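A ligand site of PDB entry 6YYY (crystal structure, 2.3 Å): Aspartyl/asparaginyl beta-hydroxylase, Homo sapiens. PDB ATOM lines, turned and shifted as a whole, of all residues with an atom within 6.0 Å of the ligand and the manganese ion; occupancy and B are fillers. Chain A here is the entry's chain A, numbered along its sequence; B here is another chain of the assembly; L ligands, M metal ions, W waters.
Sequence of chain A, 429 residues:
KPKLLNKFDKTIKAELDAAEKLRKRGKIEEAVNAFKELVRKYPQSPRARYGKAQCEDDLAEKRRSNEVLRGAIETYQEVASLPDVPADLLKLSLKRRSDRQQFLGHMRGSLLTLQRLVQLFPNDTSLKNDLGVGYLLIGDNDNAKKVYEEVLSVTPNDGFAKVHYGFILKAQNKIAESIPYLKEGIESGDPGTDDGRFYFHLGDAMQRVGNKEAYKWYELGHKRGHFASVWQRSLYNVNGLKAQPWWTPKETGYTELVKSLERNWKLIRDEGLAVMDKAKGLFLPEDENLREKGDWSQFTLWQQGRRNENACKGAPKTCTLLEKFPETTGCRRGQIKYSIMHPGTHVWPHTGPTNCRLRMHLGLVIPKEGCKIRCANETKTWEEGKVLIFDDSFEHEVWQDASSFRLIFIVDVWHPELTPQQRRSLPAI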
ATOM      1  N   LEU A 290       6.728 -12.983 -22.836  1.00  0.00           N
ATOM      2  CA  LEU A 290       7.104 -12.077 -23.915  1.00  0.00           C
ATOM      3  C   LEU A 290       8.546 -11.541 -23.919  1.00  0.00           C
ATOM      4  O   LEU A 290       8.882 -10.768 -24.824  1.00  0.00           O
ATOM      5  CB  LEU A 290       6.118 -10.893 -23.867  1.00  0.00           C
ATOM      6  CG  LEU A 290       4.718 -11.388 -24.185  1.00  0.00           C
ATOM      7  CD1 LEU A 290       3.760 -10.257 -24.368  1.00  0.00           C
ATOM      8  CD2 LEU A 290       4.630 -12.203 -25.490  1.00  0.00           C
ATOM      9  N   TRP A 296      10.677  -6.060 -16.576  1.00  0.00           N
ATOM     10  CA  TRP A 296       9.484  -5.360 -17.046  1.00  0.00           C
ATOM     11  C   TRP A 296       8.367  -5.807 -16.112  1.00  0.00           C
ATOM     12  O   TRP A 296       8.003  -7.009 -16.125  1.00  0.00           O
ATOM     13  CB  TRP A 296       9.243  -5.738 -18.505  1.00  0.00           C
ATOM     14  CG  TRP A 296       7.867  -5.494 -18.988  1.00  0.00           C
ATOM     15  CD1 TRP A 296       6.968  -4.549 -18.525  1.00  0.00           C
ATOM     16  CD2 TRP A 296       7.193  -6.209 -20.018  1.00  0.00           C
ATOM     17  NE1 TRP A 296       5.788  -4.641 -19.243  1.00  0.00           N
ATOM     18  CE2 TRP A 296       5.906  -5.672 -20.140  1.00  0.00           C
ATOM     19  CE3 TRP A 296       7.567  -7.266 -20.862  1.00  0.00           C
ATOM     20  CZ2 TRP A 296       4.950  -6.189 -21.060  1.00  0.00           C
ATOM     21  CZ3 TRP A 296       6.653  -7.706 -21.836  1.00  0.00           C
ATOM     22  CH2 TRP A 296       5.358  -7.177 -21.917  1.00  0.00           C
ATOM     23  N   GLN A 298       4.441  -4.331 -14.124  1.00  0.00           N
ATOM     24  CA  GLN A 298       3.285  -3.531 -14.527  1.00  0.00           C
ATOM     25  C   GLN A 298       2.297  -3.315 -13.369  1.00  0.00           C
ATOM     26  O   GLN A 298       1.985  -4.253 -12.637  1.00  0.00           O
ATOM     27  CB  GLN A 298       2.509  -4.213 -15.717  1.00  0.00           C
ATOM     28  CG  GLN A 298       2.955  -3.733 -17.113  1.00  0.00           C
ATOM     29  CD  GLN A 298       2.336  -4.486 -18.236  1.00  0.00           C
ATOM     30  OE1 GLN A 298       1.814  -5.586 -18.062  1.00  0.00           O
ATOM     31  NE2 GLN A 298       2.407  -3.916 -19.423  1.00  0.00           N
ATOM     32  N   LYS A 337      -2.643   0.759 -17.423  1.00  0.00           N
ATOM     33  CA  LYS A 337      -1.608   0.358 -16.479  1.00  0.00           C
ATOM     34  C   LYS A 337      -0.298   1.068 -16.726  1.00  0.00           C
ATOM     35  O   LYS A 337       0.061   1.358 -17.870  1.00  0.00           O
ATOM     36  CB  LYS A 337      -1.352  -1.148 -16.553  1.00  0.00           C
ATOM     37  CG  LYS A 337      -0.948  -1.667 -18.001  1.00  0.00           C
ATOM     38  CD  LYS A 337      -1.656  -2.983 -18.395  1.00  0.00           C
ATOM     39  CE  LYS A 337      -1.194  -3.377 -19.795  1.00  0.00           C
ATOM     40  NZ  LYS A 337      -1.261  -4.882 -19.977  1.00  0.00           N
ATOM     41  N   SER A 339       3.759   0.832 -16.824  1.00  0.00           N
ATOM     42  CA  SER A 339       4.606  -0.265 -17.302  1.00  0.00           C
ATOM     43  C   SER A 339       6.053   0.208 -17.220  1.00  0.00           C
ATOM     44  O   SER A 339       6.455   1.092 -17.982  1.00  0.00           O
ATOM     45  CB  SER A 339       4.244  -0.700 -18.727  1.00  0.00           C
ATOM     46  OG  SER A 339       5.038  -1.810 -19.144  1.00  0.00           O
ATOM     47  N   ILE A 340       6.805  -0.348 -16.287  1.00  0.00           N
ATOM     48  CA  ILE A 340       8.137   0.127 -15.967  1.00  0.00           C
ATOM     49  C   ILE A 340       9.040  -0.889 -16.607  1.00  0.00           C
ATOM     50  O   ILE A 340       8.769  -2.089 -16.458  1.00  0.00           O
ATOM     51  CB  ILE A 340       8.395   0.217 -14.449  1.00  0.00           C
ATOM     52  CG1 ILE A 340       9.854   0.647 -14.193  1.00  0.00           C
ATOM     53  CG2 ILE A 340       8.188  -1.117 -13.842  1.00  0.00           C
ATOM     54  CD1 ILE A 340      10.171   1.340 -12.919  1.00  0.00           C
ATOM     55  N   MET A 341      10.017  -0.439 -17.399  1.00  0.00           N
ATOM     56  CA  MET A 341      10.935  -1.355 -18.117  1.00  0.00           C
ATOM     57  C   MET A 341      12.380  -0.935 -17.977  1.00  0.00           C
ATOM     58  O   MET A 341      12.726   0.219 -18.256  1.00  0.00           O
ATOM     59  CB  MET A 341      10.629  -1.409 -19.607  1.00  0.00           C
ATOM     60  CG  MET A 341      11.321  -2.530 -20.312  1.00  0.00           C
ATOM     61  SD  MET A 341      11.279  -2.645 -22.155  1.00  0.00           S
ATOM     62  CE  MET A 341       9.595  -3.081 -22.475  1.00  0.00           C
ATOM     63  N   VAL A 347      11.914  -7.155 -25.864  1.00  0.00           N
ATOM     64  CA  VAL A 347      10.643  -7.858 -25.864  1.00  0.00           C
ATOM     65  C   VAL A 347      10.488  -8.489 -27.230  1.00  0.00           C
ATOM     66  O   VAL A 347      10.358  -7.770 -28.222  1.00  0.00           O
ATOM     67  CB  VAL A 347       9.457  -6.924 -25.597  1.00  0.00           C
ATOM     68  CG1 VAL A 347       8.223  -7.722 -25.524  1.00  0.00           C
ATOM     69  CG2 VAL A 347       9.598  -6.232 -24.262  1.00  0.00           C
ATOM     70  N   HIS A 350       5.759  -9.709 -31.038  1.00  0.00           N
ATOM     71  CA  HIS A 350       4.552 -10.375 -30.615  1.00  0.00           C
ATOM     72  C   HIS A 350       3.371  -9.537 -31.085  1.00  0.00           C
ATOM     73  O   HIS A 350       3.566  -8.400 -31.457  1.00  0.00           O
ATOM     74  CB  HIS A 350       4.497 -10.489 -29.089  1.00  0.00           C
ATOM     75  CG  HIS A 350       4.442  -9.142 -28.386  1.00  0.00           C
ATOM     76  ND1 HIS A 350       5.561  -8.383 -28.181  1.00  0.00           N
ATOM     77  CD2 HIS A 350       3.426  -8.387 -27.913  1.00  0.00           C
ATOM     78  CE1 HIS A 350       5.249  -7.230 -27.635  1.00  0.00           C
ATOM     79  NE2 HIS A 350       3.950  -7.181 -27.545  1.00  0.00           N
ATOM     80  N   THR A 351       2.148 -10.082 -30.883  1.00  0.00           N
ATOM     81  CA  THR A 351       0.835  -9.538 -31.196  1.00  0.00           C
ATOM     82  C   THR A 351      -0.090  -9.608 -29.976  1.00  0.00           C
ATOM     83  O   THR A 351      -0.006 -10.488 -29.162  1.00  0.00           O
ATOM     84  CB  THR A 351       0.102 -10.243 -32.447  1.00  0.00           C
ATOM     85  OG1 THR A 351       0.578  -9.674 -33.666  1.00  0.00           O
ATOM     86  N   GLY A 352      -1.023  -8.670 -29.888  1.00  0.00           N
ATOM     87  CA  GLY A 352      -2.049  -8.799 -28.930  1.00  0.00           C
ATOM     88  C   GLY A 352      -3.095  -9.735 -29.517  1.00  0.00           C
ATOM     89  O   GLY A 352      -2.954 -10.299 -30.587  1.00  0.00           O
ATOM     90  N   ARG A 359      -4.012   1.266 -28.636  1.00  0.00           N
ATOM     91  CA  ARG A 359      -3.176   1.314 -27.447  1.00  0.00           C
ATOM     92  C   ARG A 359      -2.472   2.649 -27.393  1.00  0.00           C
ATOM     93  O   ARG A 359      -1.716   2.975 -28.318  1.00  0.00           O
ATOM     94  CB  ARG A 359      -2.183   0.179 -27.491  1.00  0.00           C
ATOM     95  CG  ARG A 359      -1.321   0.075 -26.282  1.00  0.00           C
ATOM     96  CD  ARG A 359      -1.024  -1.389 -26.063  1.00  0.00           C
ATOM     97  NE  ARG A 359      -1.826  -2.002 -24.987  1.00  0.00           N
ATOM     98  CZ  ARG A 359      -1.654  -3.243 -24.561  1.00  0.00           C
ATOM     99  NH1 ARG A 359      -2.382  -3.682 -23.548  1.00  0.00           N
ATOM    100  NH2 ARG A 359      -0.649  -4.012 -25.043  1.00  0.00           N
ATOM    101  N   HIS A 361       0.211   5.009 -25.462  1.00  0.00           N
ATOM    102  CA  HIS A 361       1.333   5.171 -24.586  1.00  0.00           C
ATOM    103  C   HIS A 361       1.522   6.632 -24.211  1.00  0.00           C
ATOM    104  O   HIS A 361       1.424   7.516 -25.056  1.00  0.00           O
ATOM    105  CB  HIS A 361       2.550   4.629 -25.310  1.00  0.00           C
ATOM    106  CG  HIS A 361       2.638   3.144 -25.278  1.00  0.00           C
ATOM    107  ND1 HIS A 361       3.660   2.462 -25.886  1.00  0.00           N
ATOM    108  CD2 HIS A 361       1.879   2.215 -24.667  1.00  0.00           C
ATOM    109  CE1 HIS A 361       3.525   1.174 -25.663  1.00  0.00           C
ATOM    110  NE2 HIS A 361       2.439   0.992 -24.939  1.00  0.00           N
ATOM    111  N   ILE A 373      10.708   1.209 -29.908  1.00  0.00           N
ATOM    112  CA  ILE A 373       9.578   0.299 -30.115  1.00  0.00           C
ATOM    113  C   ILE A 373       9.344   0.209 -31.618  1.00  0.00           C
ATOM    114  O   ILE A 373       9.384   1.225 -32.330  1.00  0.00           O
ATOM    115  CB  ILE A 373       8.284   0.803 -29.457  1.00  0.00           C
ATOM    116  CG1 ILE A 373       7.100  -0.053 -29.933  1.00  0.00           C
ATOM    117  CG2 ILE A 373       8.121   2.286 -29.864  1.00  0.00           C
ATOM    118  CD1 ILE A 373       5.819   0.001 -29.064  1.00  0.00           C
ATOM    119  N   TRP A 382       9.342   7.085 -27.332  1.00  0.00           N
ATOM    120  CA  TRP A 382       8.457   7.915 -26.507  1.00  0.00           C
ATOM    121  C   TRP A 382       9.030   9.323 -26.256  1.00  0.00           C
ATOM    122  O   TRP A 382      10.225   9.569 -26.395  1.00  0.00           O
ATOM    123  CB  TRP A 382       8.216   7.227 -25.161  1.00  0.00           C
ATOM    124  CG  TRP A 382       7.601   5.866 -25.367  1.00  0.00           C
ATOM    125  CD1 TRP A 382       6.292   5.587 -25.469  1.00  0.00           C
ATOM    126  CD2 TRP A 382       8.274   4.634 -25.527  1.00  0.00           C
ATOM    127  NE1 TRP A 382       6.090   4.260 -25.706  1.00  0.00           N
ATOM    128  CE2 TRP A 382       7.303   3.648 -25.727  1.00  0.00           C
ATOM    129  CE3 TRP A 382       9.605   4.250 -25.490  1.00  0.00           C
ATOM    130  CZ2 TRP A 382       7.610   2.340 -25.895  1.00  0.00           C
ATOM    131  CZ3 TRP A 382       9.915   2.967 -25.675  1.00  0.00           C
ATOM    132  CH2 TRP A 382       8.935   2.021 -25.859  1.00  0.00           C
ATOM    133  N   PHE A 390      -0.833   3.005 -31.129  1.00  0.00           N
ATOM    134  CA  PHE A 390      -0.633   2.035 -32.189  1.00  0.00           C
ATOM    135  C   PHE A 390      -1.689   0.955 -32.068  1.00  0.00           C
ATOM    136  O   PHE A 390      -2.445   0.891 -31.078  1.00  0.00           O
ATOM    137  CB  PHE A 390       0.797   1.449 -32.146  1.00  0.00           C
ATOM    138  CG  PHE A 390       1.079   0.545 -30.959  1.00  0.00           C
ATOM    139  CD1 PHE A 390       1.391   1.070 -29.711  1.00  0.00           C
ATOM    140  CD2 PHE A 390       1.121  -0.830 -31.098  1.00  0.00           C
ATOM    141  CE1 PHE A 390       1.675   0.232 -28.664  1.00  0.00           C
ATOM    142  CE2 PHE A 390       1.383  -1.652 -30.025  1.00  0.00           C
ATOM    143  CZ  PHE A 390       1.649  -1.116 -28.825  1.00  0.00           C
ATOM    144  N   ASP A 392      -2.016  -2.562 -31.423  1.00  0.00           N
ATOM    145  CA  ASP A 392      -1.237  -3.664 -30.880  1.00  0.00           C
ATOM    146  C   ASP A 392      -1.606  -5.012 -31.504  1.00  0.00           C
ATOM    147  O   ASP A 392      -0.862  -5.977 -31.285  1.00  0.00           O
ATOM    148  CB  ASP A 392      -1.360  -3.726 -29.348  1.00  0.00           C
ATOM    149  CG  ASP A 392      -2.397  -4.739 -28.837  1.00  0.00           C
ATOM    150  OD1 ASP A 392      -3.330  -5.160 -29.582  1.00  0.00           O
ATOM    151  OD2 ASP A 392      -2.241  -5.089 -27.623  1.00  0.00           O
ATOM    152  N   HIS A 396       4.689  -5.900 -32.782  1.00  0.00           N
ATOM    153  CA  HIS A 396       5.523  -4.888 -32.139  1.00  0.00           C
ATOM    154  C   HIS A 396       6.625  -5.560 -31.305  1.00  0.00           C
ATOM    155  O   HIS A 396       6.501  -6.700 -30.844  1.00  0.00           O
ATOM    156  CB  HIS A 396       4.673  -3.884 -31.269  1.00  0.00           C
ATOM    157  CG  HIS A 396       3.625  -4.554 -30.434  1.00  0.00           C
ATOM    158  ND1 HIS A 396       2.519  -5.150 -30.976  1.00  0.00           N
ATOM    159  CD2 HIS A 396       3.533  -4.741 -29.099  1.00  0.00           C
ATOM    160  CE1 HIS A 396       1.802  -5.709 -30.016  1.00  0.00           C
ATOM    161  NE2 HIS A 396       2.398  -5.477 -28.872  1.00  0.00           N
ATOM    162  N   VAL A 398      10.253  -4.389 -28.750  1.00  0.00           N
ATOM    163  CA  VAL A 398      10.770  -3.295 -27.913  1.00  0.00           C
ATOM    164  C   VAL A 398      12.158  -3.663 -27.413  1.00  0.00           C
ATOM    165  O   VAL A 398      12.466  -4.828 -27.173  1.00  0.00           O
ATOM    166  CB  VAL A 398       9.854  -2.996 -26.707  1.00  0.00           C
ATOM    167  CG1 VAL A 398      10.528  -2.015 -25.764  1.00  0.00           C
ATOM    168  CG2 VAL A 398       8.497  -2.422 -27.181  1.00  0.00           C
ATOM    169  N   ARG A 406      12.666   3.188 -17.412  1.00  0.00           N
ATOM    170  CA  ARG A 406      11.788   3.841 -18.377  1.00  0.00           C
ATOM    171  C   ARG A 406      10.368   3.506 -18.013  1.00  0.00           C
ATOM    172  O   ARG A 406      10.006   2.320 -17.986  1.00  0.00           O
ATOM    173  CB  ARG A 406      11.994   3.349 -19.820  1.00  0.00           C
ATOM    174  CG  ARG A 406      11.132   4.092 -20.851  1.00  0.00           C
ATOM    175  CD  ARG A 406      10.292   3.176 -21.690  1.00  0.00           C
ATOM    176  NE  ARG A 406       9.466   2.267 -20.879  1.00  0.00           N
ATOM    177  CZ  ARG A 406       8.694   1.312 -21.402  1.00  0.00           C
ATOM    178  NH1 ARG A 406       8.590   1.157 -22.711  1.00  0.00           N
ATOM    179  NH2 ARG A 406       7.975   0.527 -20.643  1.00  0.00           N
ATOM    180  N   ILE A 408       6.080   4.488 -18.678  1.00  0.00           N
ATOM    181  CA  ILE A 408       5.027   4.969 -19.546  1.00  0.00           C
ATOM    182  C   ILE A 408       3.702   4.557 -18.928  1.00  0.00           C
ATOM    183  O   ILE A 408       3.644   3.694 -18.054  1.00  0.00           O
ATOM    184  CB  ILE A 408       5.157   4.360 -20.963  1.00  0.00           C
ATOM    185  CG1 ILE A 408       5.022   2.847 -20.904  1.00  0.00           C
ATOM    186  CG2 ILE A 408       6.531   4.708 -21.612  1.00  0.00           C
ATOM    187  CD1 ILE A 408       4.846   2.222 -22.316  1.00  0.00           C
ATOM    188  N   ILE A 410      -0.097   3.138 -20.113  1.00  0.00           N
ATOM    189  CA  ILE A 410      -0.779   2.462 -21.211  1.00  0.00           C
ATOM    190  C   ILE A 410      -2.260   2.537 -20.964  1.00  0.00           C
ATOM    191  O   ILE A 410      -2.742   2.102 -19.910  1.00  0.00           O
ATOM    192  CB  ILE A 410      -0.349   0.994 -21.315  1.00  0.00           C
ATOM    193  CG1 ILE A 410       1.148   0.924 -21.185  1.00  0.00           C
ATOM    194  CG2 ILE A 410      -0.923   0.332 -22.582  1.00  0.00           C
ATOM    195  CD1 ILE A 410       1.530  -0.466 -20.854  1.00  0.00           C
ATOM    196  N   ASP B  18      -1.319  -8.898 -23.324  1.00  0.00           N
ATOM    197  CA  ASP B  18      -0.468  -8.353 -24.360  1.00  0.00           C
ATOM    198  C   ASP B  18      -0.188  -9.347 -25.460  1.00  0.00           C
ATOM    199  O   ASP B  18       0.381  -8.942 -26.468  1.00  0.00           O
ATOM    200  CB  ASP B  18       0.872  -7.929 -23.762  1.00  0.00           C
ATOM    201  CG  ASP B  18       0.758  -6.762 -22.812  1.00  0.00           C
ATOM    202  OD1 ASP B  18      -0.369  -6.330 -22.483  1.00  0.00           O
ATOM    203  OD2 ASP B  18       1.821  -6.227 -22.450  1.00  0.00           O
HETATM  204  C1  LIG L   1       2.430  -2.886 -25.254  1.00  0.00           C
HETATM  205  C2  LIG L   1       3.629  -3.304 -24.841  1.00  0.00           C
HETATM  206  C3  LIG L   1       4.179  -2.602 -23.557  1.00  0.00           C
HETATM  207  C4  LIG L   1       5.677  -2.690 -23.277  1.00  0.00           C
HETATM  208  C5  LIG L   1       6.319  -1.444 -22.701  1.00  0.00           C
HETATM  209  C6  LIG L   1       5.891  -3.672 -22.171  1.00  0.00           C
HETATM  210  C7  LIG L   1       6.506  -3.272 -24.415  1.00  0.00           C
HETATM  211  O1  LIG L   1       4.080  -4.242 -25.545  1.00  0.00           O
HETATM  212  O2  LIG L   1       1.960  -3.314 -26.411  1.00  0.00           O
HETATM  213  O3  LIG L   1       1.747  -2.170 -24.568  1.00  0.00           O
HETATM  214  O4  LIG L   1       6.113  -1.020 -21.414  1.00  0.00           O
HETATM  215  O5  LIG L   1       7.147  -0.851 -23.375  1.00  0.00           O
HETATM  216 MN    MN M   1       2.474  -5.531 -26.548  1.00  0.00          MN
HETATM  217  O   HOH W   1       0.278  -5.933 -27.224  1.00  0.00           O
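The side-chain hydroxyl (OG) of Ser 339 lies within hydrogen-bond range of an oxygen (O4) of the ligand (2.6 Å). An oxygen (O4) of the ligand is in salt-bridge range of the guanidinium group of Arg 406 (2.5 Å). An oxygen (O3) of the ligand is in salt-bridge range of the guanidinium group of Arg 359, 3.1 Å away. An oxygen (O3) of the ligand lies within hydrogen-bond range of a ring nitrogen (NE2) of His 361 (3.3 Å).
NH2 of Arg 359 lies within salt-bridge range of OD1 of Asp 18 of chain B (3.5 Å). The guanidinium group (NH2) of Arg 406 sits at hydrogen-bond distance from the backbone carbonyl oxygen (O) of Ser 339 (3.1 Å). The guanidinium group (NH2) of Arg 359 lies within salt-bridge range of the side-chain carboxylate (OD2) of Asp 392 (3.2 Å). O of Ile 408 sits at hydrogen-bond distance from N of Ser 339 (3.1 Å). The backbone carbonyl oxygen of Arg 406 lies within hydrogen-bond range of the backbone NH of Met 341 (2.8 Å). OG of Ser 339 sits at hydrogen-bond distance from NE1 of Trp 296, 2.9 Å away. The backbone NH (N) of Arg 359 lies within hydrogen-bond range of the backbone carbonyl oxygen (O) of Phe 390 (2.9 Å). O of Asp 392 lies close to ND1 of His 396 (3.5 Å).
Trp 296 touches the ligand (CE2 to C6, 2.9 Å). CE of Met 341 touches O5 of the ligand, at 3.4 Å. CZ of Phe 390 touches O2 of the ligand (3.3 Å). Val 398 touches the ligand (CG2 to C7, 3.5 Å). Ile 408 touches the ligand (CD1 to O4, 3.6 Å). 11 residues have an atom within 4 Å of the ligand: Trp 296, Ser 339, Met 341, His 350, Arg 359, His 361, Phe 390, His 396, Val 398, Arg 406 and Ile 408. The nearest printed residue that does not touch the ligand is Ile 410 (4.1 Å).
Arg 359 touches the manganese ion (NH2 to MN, 3.8 Å). Three residues have an atom within 4 Å of the manganese ion: His 350, Arg 359 and His 396. The nearest printed residue that does not touch the manganese ion is Asp 18 of chain B (4.003 Å).
The manganese ion is bound by O2 of the ligand (2.3 Å), O1 of the ligand (2.3 Å), NE2 of His 396 (2.3 Å), water W1 (2.3 Å) and NE2 of His 350 (2.4 Å). The manganese ion has five donor atoms within binding distance.
Water W1 lies within hydrogen-bond range of the side-chain carboxylate (OD2) of Asp 392 (2.7 Å), the guanidinium group (NH2) of Arg 359 (3.1 Å) and the backbone carbonyl oxygen (O) of Asp 18 of chain B (3.1 Å).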
